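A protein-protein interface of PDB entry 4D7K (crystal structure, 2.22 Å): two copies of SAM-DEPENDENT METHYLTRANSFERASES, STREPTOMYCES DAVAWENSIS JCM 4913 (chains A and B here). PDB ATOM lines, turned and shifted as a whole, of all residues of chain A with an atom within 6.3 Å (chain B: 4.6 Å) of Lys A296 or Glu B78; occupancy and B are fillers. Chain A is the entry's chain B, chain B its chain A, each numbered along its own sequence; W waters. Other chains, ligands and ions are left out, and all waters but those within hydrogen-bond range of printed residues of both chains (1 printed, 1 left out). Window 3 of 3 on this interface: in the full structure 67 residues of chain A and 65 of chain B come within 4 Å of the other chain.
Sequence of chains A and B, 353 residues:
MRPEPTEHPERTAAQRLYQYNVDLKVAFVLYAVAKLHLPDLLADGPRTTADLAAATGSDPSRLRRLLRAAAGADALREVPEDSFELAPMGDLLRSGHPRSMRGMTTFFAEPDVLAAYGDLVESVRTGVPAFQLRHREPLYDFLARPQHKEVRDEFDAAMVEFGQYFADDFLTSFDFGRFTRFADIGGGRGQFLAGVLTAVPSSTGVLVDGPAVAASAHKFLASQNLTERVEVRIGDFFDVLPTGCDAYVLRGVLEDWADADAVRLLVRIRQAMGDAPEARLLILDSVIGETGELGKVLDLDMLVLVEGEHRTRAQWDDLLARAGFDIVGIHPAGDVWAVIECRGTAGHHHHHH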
ATOM      1  N   SER A 286      30.889 -22.288  24.463  1.00  0.00           N
ATOM      2  CA  SER A 286      30.458 -21.807  23.153  1.00  0.00           C
ATOM      3  C   SER A 286      28.973 -22.124  22.963  1.00  0.00           C
ATOM      4  O   SER A 286      28.574 -23.288  23.018  1.00  0.00           O
ATOM      5  CB  SER A 286      31.296 -22.449  22.041  1.00  0.00           C
ATOM      6  OG  SER A 286      31.068 -21.820  20.794  1.00  0.00           O
ATOM      7  N   GLY A 289      24.338 -20.708  17.985  1.00  0.00           N
ATOM      8  CA  GLY A 289      23.426 -19.678  17.523  1.00  0.00           C
ATOM      9  C   GLY A 289      23.779 -18.312  18.080  1.00  0.00           C
ATOM     10  O   GLY A 289      23.330 -17.286  17.572  1.00  0.00           O
ATOM     11  N   THR A 291      27.203 -17.673  18.928  1.00  0.00           N
ATOM     12  CA  THR A 291      28.650 -17.597  18.825  1.00  0.00           C
ATOM     13  C   THR A 291      28.980 -16.811  17.563  1.00  0.00           C
ATOM     14  O   THR A 291      28.109 -16.595  16.724  1.00  0.00           O
ATOM     15  CB  THR A 291      29.302 -18.997  18.782  1.00  0.00           C
ATOM     16  OG1 THR A 291      30.724 -18.868  18.895  1.00  0.00           O
ATOM     17  CG2 THR A 291      28.960 -19.720  17.484  1.00  0.00           C
ATOM     18  N   GLY A 292      30.224 -16.368  17.429  1.00  0.00           N
ATOM     19  CA  GLY A 292      30.634 -15.652  16.233  1.00  0.00           C
ATOM     20  C   GLY A 292      31.005 -16.620  15.125  1.00  0.00           C
ATOM     21  O   GLY A 292      30.931 -17.832  15.310  1.00  0.00           O
ATOM     22  N   GLU A 293      31.413 -16.086  13.978  1.00  0.00           N
ATOM     23  CA  GLU A 293      31.831 -16.915  12.853  1.00  0.00           C
ATOM     24  C   GLU A 293      33.000 -17.831  13.219  1.00  0.00           C
ATOM     25  O   GLU A 293      33.060 -18.982  12.784  1.00  0.00           O
ATOM     26  CB  GLU A 293      32.205 -16.032  11.659  1.00  0.00           C
ATOM     27  CG  GLU A 293      31.093 -15.075  11.229  1.00  0.00           C
ATOM     28  CD  GLU A 293      29.739 -15.761  11.096  1.00  0.00           C
ATOM     29  OE1 GLU A 293      29.529 -16.504  10.112  1.00  0.00           O
ATOM     30  OE2 GLU A 293      28.883 -15.559  11.984  1.00  0.00           O
ATOM     31  N   LEU A 294      33.926 -17.317  14.022  1.00  0.00           N
ATOM     32  CA  LEU A 294      35.070 -18.106  14.464  1.00  0.00           C
ATOM     33  C   LEU A 294      34.613 -19.299  15.294  1.00  0.00           C
ATOM     34  O   LEU A 294      35.169 -20.389  15.185  1.00  0.00           O
ATOM     35  CB  LEU A 294      36.045 -17.239  15.264  1.00  0.00           C
ATOM     36  CG  LEU A 294      37.282 -17.939  15.829  1.00  0.00           C
ATOM     37  CD1 LEU A 294      38.079 -18.627  14.733  1.00  0.00           C
ATOM     38  CD2 LEU A 294      38.152 -16.948  16.583  1.00  0.00           C
ATOM     39  N   GLY A 295      33.586 -19.090  16.114  1.00  0.00           N
ATOM     40  CA  GLY A 295      33.046 -20.152  16.943  1.00  0.00           C
ATOM     41  C   GLY A 295      32.460 -21.298  16.138  1.00  0.00           C
ATOM     42  O   GLY A 295      32.570 -22.459  16.526  1.00  0.00           O
ATOM     43  N   LYS A 296      31.831 -20.971  15.013  1.00  0.00           N
ATOM     44  CA  LYS A 296      31.246 -21.981  14.142  1.00  0.00           C
ATOM     45  C   LYS A 296      32.333 -22.843  13.503  1.00  0.00           C
ATOM     46  O   LYS A 296      32.153 -24.047  13.319  1.00  0.00           O
ATOM     47  CB  LYS A 296      30.384 -21.319  13.061  1.00  0.00           C
ATOM     48  CG  LYS A 296      29.257 -20.444  13.605  1.00  0.00           C
ATOM     49  CD  LYS A 296      28.553 -19.697  12.486  1.00  0.00           C
ATOM     50  CE  LYS A 296      27.451 -18.809  13.028  1.00  0.00           C
ATOM     51  NZ  LYS A 296      26.894 -17.919  11.975  1.00  0.00           N
ATOM     52  N   VAL A 297      33.463 -22.221  13.175  1.00  0.00           N
ATOM     53  CA  VAL A 297      34.612 -22.936  12.631  1.00  0.00           C
ATOM     54  C   VAL A 297      35.247 -23.860  13.666  1.00  0.00           C
ATOM     55  O   VAL A 297      35.591 -24.999  13.360  1.00  0.00           O
ATOM     56  CB  VAL A 297      35.686 -21.959  12.112  1.00  0.00           C
ATOM     57  CG1 VAL A 297      36.934 -22.716  11.688  1.00  0.00           C
ATOM     58  CG2 VAL A 297      35.137 -21.132  10.961  1.00  0.00           C
ATOM     59  N   LEU A 298      35.394 -23.368  14.894  1.00  0.00           N
ATOM     60  CA  LEU A 298      36.066 -24.126  15.948  1.00  0.00           C
ATOM     61  C   LEU A 298      35.286 -25.366  16.372  1.00  0.00           C
ATOM     62  O   LEU A 298      35.845 -26.275  16.986  1.00  0.00           O
ATOM     63  CB  LEU A 298      36.319 -23.239  17.171  1.00  0.00           C
ATOM     64  CG  LEU A 298      37.402 -22.167  17.042  1.00  0.00           C
ATOM     65  CD1 LEU A 298      37.703 -21.571  18.398  1.00  0.00           C
ATOM     66  CD2 LEU A 298      38.666 -22.727  16.421  1.00  0.00           C
ATOM     67  N   ASP A 299      33.998 -25.405  16.040  1.00  0.00           N
ATOM     68  CA  ASP A 299      33.161 -26.555  16.363  1.00  0.00           C
ATOM     69  C   ASP A 299      33.629 -27.771  15.569  1.00  0.00           C
ATOM     70  O   ASP A 299      33.273 -28.906  15.883  1.00  0.00           O
ATOM     71  CB  ASP A 299      31.687 -26.252  16.068  1.00  0.00           C
ATOM     72  CG  ASP A 299      30.736 -27.284  16.676  1.00  0.00           C
ATOM     73  OD1 ASP A 299      30.964 -27.709  17.828  1.00  0.00           O
ATOM     74  OD2 ASP A 299      29.749 -27.663  16.004  1.00  0.00           O
ATOM     75  N   LEU A 300      34.428 -27.521  14.536  1.00  0.00           N
ATOM     76  CA  LEU A 300      35.070 -28.585  13.776  1.00  0.00           C
ATOM     77  C   LEU A 300      35.921 -29.481  14.678  1.00  0.00           C
ATOM     78  O   LEU A 300      35.970 -30.700  14.488  1.00  0.00           O
ATOM     79  CB  LEU A 300      35.935 -27.997  12.663  1.00  0.00           C
ATOM     80  CG  LEU A 300      36.748 -29.031  11.890  1.00  0.00           C
ATOM     81  CD1 LEU A 300      35.803 -29.985  11.195  1.00  0.00           C
ATOM     82  CD2 LEU A 300      37.688 -28.371  10.899  1.00  0.00           C
ATOM     83  N   ASP A 335      34.878 -13.740  20.081  1.00  0.00           N
ATOM     84  CA  ASP A 335      34.177 -14.236  18.903  1.00  0.00           C
ATOM     85  C   ASP A 335      33.779 -15.703  19.024  1.00  0.00           C
ATOM     86  O   ASP A 335      33.181 -16.265  18.108  1.00  0.00           O
ATOM     87  CB  ASP A 335      35.044 -14.043  17.658  1.00  0.00           C
ATOM     88  CG  ASP A 335      35.349 -12.583  17.378  1.00  0.00           C
ATOM     89  OD1 ASP A 335      34.593 -11.710  17.860  1.00  0.00           O
ATOM     90  OD2 ASP A 335      36.340 -12.310  16.670  1.00  0.00           O
ATOM     91  N   ARG B  68      27.451 -25.165   8.868  1.00  0.00           N
ATOM     92  CA  ARG B  68      27.552 -23.942   9.652  1.00  0.00           C
ATOM     93  C   ARG B  68      29.010 -23.466   9.747  1.00  0.00           C
ATOM     94  O   ARG B  68      29.278 -22.263   9.751  1.00  0.00           O
ATOM     95  CB  ARG B  68      26.952 -24.173  11.035  1.00  0.00           C
ATOM     96  CG  ARG B  68      26.975 -22.993  11.961  1.00  0.00           C
ATOM     97  CD  ARG B  68      26.399 -23.398  13.299  1.00  0.00           C
ATOM     98  NE  ARG B  68      25.004 -23.817  13.193  1.00  0.00           N
ATOM     99  CZ  ARG B  68      24.464 -24.791  13.917  1.00  0.00           C
ATOM    100  NH1 ARG B  68      25.207 -25.460  14.789  1.00  0.00           N
ATOM    101  NH2 ARG B  68      23.185 -25.102  13.765  1.00  0.00           N
ATOM    102  N   ALA B  69      29.950 -24.412   9.793  1.00  0.00           N
ATOM    103  CA  ALA B  69      31.374 -24.073   9.841  1.00  0.00           C
ATOM    104  C   ALA B  69      31.816 -23.454   8.521  1.00  0.00           C
ATOM    105  O   ALA B  69      32.560 -22.476   8.499  1.00  0.00           O
ATOM    106  CB  ALA B  69      32.220 -25.311  10.171  1.00  0.00           C
ATOM    107  N   ALA B  71      29.918 -21.805   6.643  1.00  0.00           N
ATOM    108  CA  ALA B  71      29.335 -20.469   6.677  1.00  0.00           C
ATOM    109  C   ALA B  71      30.248 -19.503   7.444  1.00  0.00           C
ATOM    110  O   ALA B  71      30.510 -18.385   6.988  1.00  0.00           O
ATOM    111  CB  ALA B  71      27.942 -20.510   7.301  1.00  0.00           C
ATOM    112  N   GLY B  72      30.735 -19.941   8.602  1.00  0.00           N
ATOM    113  CA  GLY B  72      31.664 -19.151   9.392  1.00  0.00           C
ATOM    114  C   GLY B  72      32.907 -18.753   8.617  1.00  0.00           C
ATOM    115  O   GLY B  72      33.448 -17.661   8.803  1.00  0.00           O
ATOM    116  N   LEU B  76      29.815 -20.580   2.494  1.00  0.00           N
ATOM    117  CA  LEU B  76      28.367 -20.646   2.314  1.00  0.00           C
ATOM    118  C   LEU B  76      27.698 -19.518   3.098  1.00  0.00           C
ATOM    119  O   LEU B  76      28.370 -18.765   3.802  1.00  0.00           O
ATOM    120  CB  LEU B  76      27.815 -21.996   2.776  1.00  0.00           C
ATOM    121  CG  LEU B  76      28.376 -23.318   2.232  1.00  0.00           C
ATOM    122  CD1 LEU B  76      27.706 -24.479   2.938  1.00  0.00           C
ATOM    123  CD2 LEU B  76      28.169 -23.446   0.740  1.00  0.00           C
ATOM    124  N   ARG B  77      26.379 -19.411   2.969  1.00  0.00           N
ATOM    125  CA  ARG B  77      25.579 -18.494   3.782  1.00  0.00           C
ATOM    126  C   ARG B  77      24.451 -19.248   4.469  1.00  0.00           C
ATOM    127  O   ARG B  77      23.783 -20.070   3.846  1.00  0.00           O
ATOM    128  CB  ARG B  77      24.979 -17.365   2.938  1.00  0.00           C
ATOM    129  CG  ARG B  77      25.953 -16.301   2.495  1.00  0.00           C
ATOM    130  CD  ARG B  77      25.197 -15.098   1.951  1.00  0.00           C
ATOM    131  NE  ARG B  77      24.370 -15.440   0.796  1.00  0.00           N
ATOM    132  CZ  ARG B  77      24.741 -15.246  -0.463  1.00  0.00           C
ATOM    133  NH1 ARG B  77      25.924 -14.707  -0.726  1.00  0.00           N
ATOM    134  NH2 ARG B  77      23.929 -15.579  -1.460  1.00  0.00           N
ATOM    135  N   GLU B  78      24.234 -18.970   5.747  1.00  0.00           N
ATOM    136  CA  GLU B  78      23.079 -19.517   6.439  1.00  0.00           C
ATOM    137  C   GLU B  78      21.831 -18.777   5.975  1.00  0.00           C
ATOM    138  O   GLU B  78      21.860 -17.565   5.787  1.00  0.00           O
ATOM    139  CB  GLU B  78      23.244 -19.409   7.952  1.00  0.00           C
ATOM    140  CG  GLU B  78      24.310 -20.321   8.517  1.00  0.00           C
ATOM    141  CD  GLU B  78      24.294 -20.357  10.028  1.00  0.00           C
ATOM    142  OE1 GLU B  78      23.364 -20.967  10.599  1.00  0.00           O
ATOM    143  OE2 GLU B  78      25.212 -19.776  10.644  1.00  0.00           O
ATOM    144  N   VAL B  79      20.741 -19.513   5.792  1.00  0.00           N
ATOM    145  CA  VAL B  79      19.521 -18.970   5.211  1.00  0.00           C
ATOM    146  C   VAL B  79      18.302 -19.510   5.964  1.00  0.00           C
ATOM    147  O   VAL B  79      18.259 -20.699   6.287  1.00  0.00           O
ATOM    148  CB  VAL B  79      19.441 -19.318   3.699  1.00  0.00           C
ATOM    149  CG1 VAL B  79      18.002 -19.403   3.204  1.00  0.00           C
ATOM    150  CG2 VAL B  79      20.252 -18.319   2.886  1.00  0.00           C
ATOM    151  N   PRO B  80      17.320 -18.633   6.261  1.00  0.00           N
ATOM    152  CA  PRO B  80      16.115 -18.952   7.040  1.00  0.00           C
ATOM    153  C   PRO B  80      15.475 -20.298   6.706  1.00  0.00           C
ATOM    154  O   PRO B  80      15.468 -20.716   5.546  1.00  0.00           O
ATOM    155  CB  PRO B  80      15.152 -17.798   6.694  1.00  0.00           C
ATOM    156  CG  PRO B  80      15.867 -16.942   5.668  1.00  0.00           C
ATOM    157  CD  PRO B  80      17.324 -17.219   5.857  1.00  0.00           C
ATOM    158  N   SER B  83      18.537 -23.560   6.224  1.00  0.00           N
ATOM    159  CA  SER B  83      18.996 -23.720   4.849  1.00  0.00           C
ATOM    160  C   SER B  83      20.370 -23.103   4.626  1.00  0.00           C
ATOM    161  O   SER B  83      20.861 -22.339   5.452  1.00  0.00           O
ATOM    162  CB  SER B  83      17.990 -23.099   3.874  1.00  0.00           C
ATOM    163  OG  SER B  83      16.741 -23.766   3.928  1.00  0.00           O
ATOM    164  N   PHE B  84      20.987 -23.448   3.498  1.00  0.00           N
ATOM    165  CA  PHE B  84      22.271 -22.875   3.133  1.00  0.00           C
ATOM    166  C   PHE B  84      22.306 -22.564   1.650  1.00  0.00           C
ATOM    167  O   PHE B  84      21.621 -23.205   0.858  1.00  0.00           O
ATOM    168  CB  PHE B  84      23.413 -23.824   3.513  1.00  0.00           C
ATOM    169  CG  PHE B  84      23.509 -24.081   4.991  1.00  0.00           C
ATOM    170  CD1 PHE B  84      22.774 -25.097   5.581  1.00  0.00           C
ATOM    171  CD2 PHE B  84      24.316 -23.291   5.789  1.00  0.00           C
ATOM    172  CE1 PHE B  84      22.844 -25.321   6.942  1.00  0.00           C
ATOM    173  CE2 PHE B  84      24.397 -23.514   7.155  1.00  0.00           C
ATOM    174  CZ  PHE B  84      23.660 -24.531   7.733  1.00  0.00           C
HETATM  175  O   HOH W   1      29.319 -16.102   7.466  1.00  0.00           O
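O of Ala B71 touches OE1 of Glu A293 (3.8 Å).
OE1 of Glu A293 touches CA of Gly B72, at 3.5 Å.
Lys A296 touches Arg B68.
Lys A296 touches Ala B69 (O to CB, 3.4 Å).
Ala B69 touches Val A297 (O to CG2, 3.8 Å).
The side-chain amino group (NZ) of Lys A296 is in salt-bridge range of the side-chain carboxylate (OE2) of Glu B78, at 2.8 Å.
Thr A291 touches none of the printed residues of chain B.
Of the printed residues of chain B, Glu A293 touches Ala B71 and Gly B72.
Of chain B, only Arg B68, Ala B69 and Glu B78 come within 4 Å of Lys A296.
Of the printed residues of chain B, Val A297 touches Ala B69.
Asp A335 touches none of the printed residues of chain B.
Of the printed residues of chain A, Arg B68 touches Lys A296.
Of the printed residues of chain A, Gly B72 touches Glu A293.
The nearest residue of chain B that does not touch Lys A296 is Gly B72 (4.4 Å).
Of the 11 printed residues of chain B, 5 touch a printed residue of chain A.
Printed residues of chain A that touch a printed residue of chain B: Glu A293, Lys A296 and Val A297.
Hydrophobic or aromatic side chains of chain A within 4 Å of the printed part of chain B: Val A297.
Among the printed residues, Asp or Glu carboxylates within 4 Å of a Lys or Arg side-chain nitrogen of the other chain: Lys A296 with Glu B78 (2.8 Å).
No position is printed for both chains.
Of the 6 pairs that touch across the chains among the printed residues, none has its exchanged pair printed and touching as well.
Water W1 bridges O of Ala B71 (2.6 Å) and OE1 of Glu A293 (2.7 Å).
OE2 of Glu A293 lies within salt-bridge range of NZ of Lys A296 (3.1 Å).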
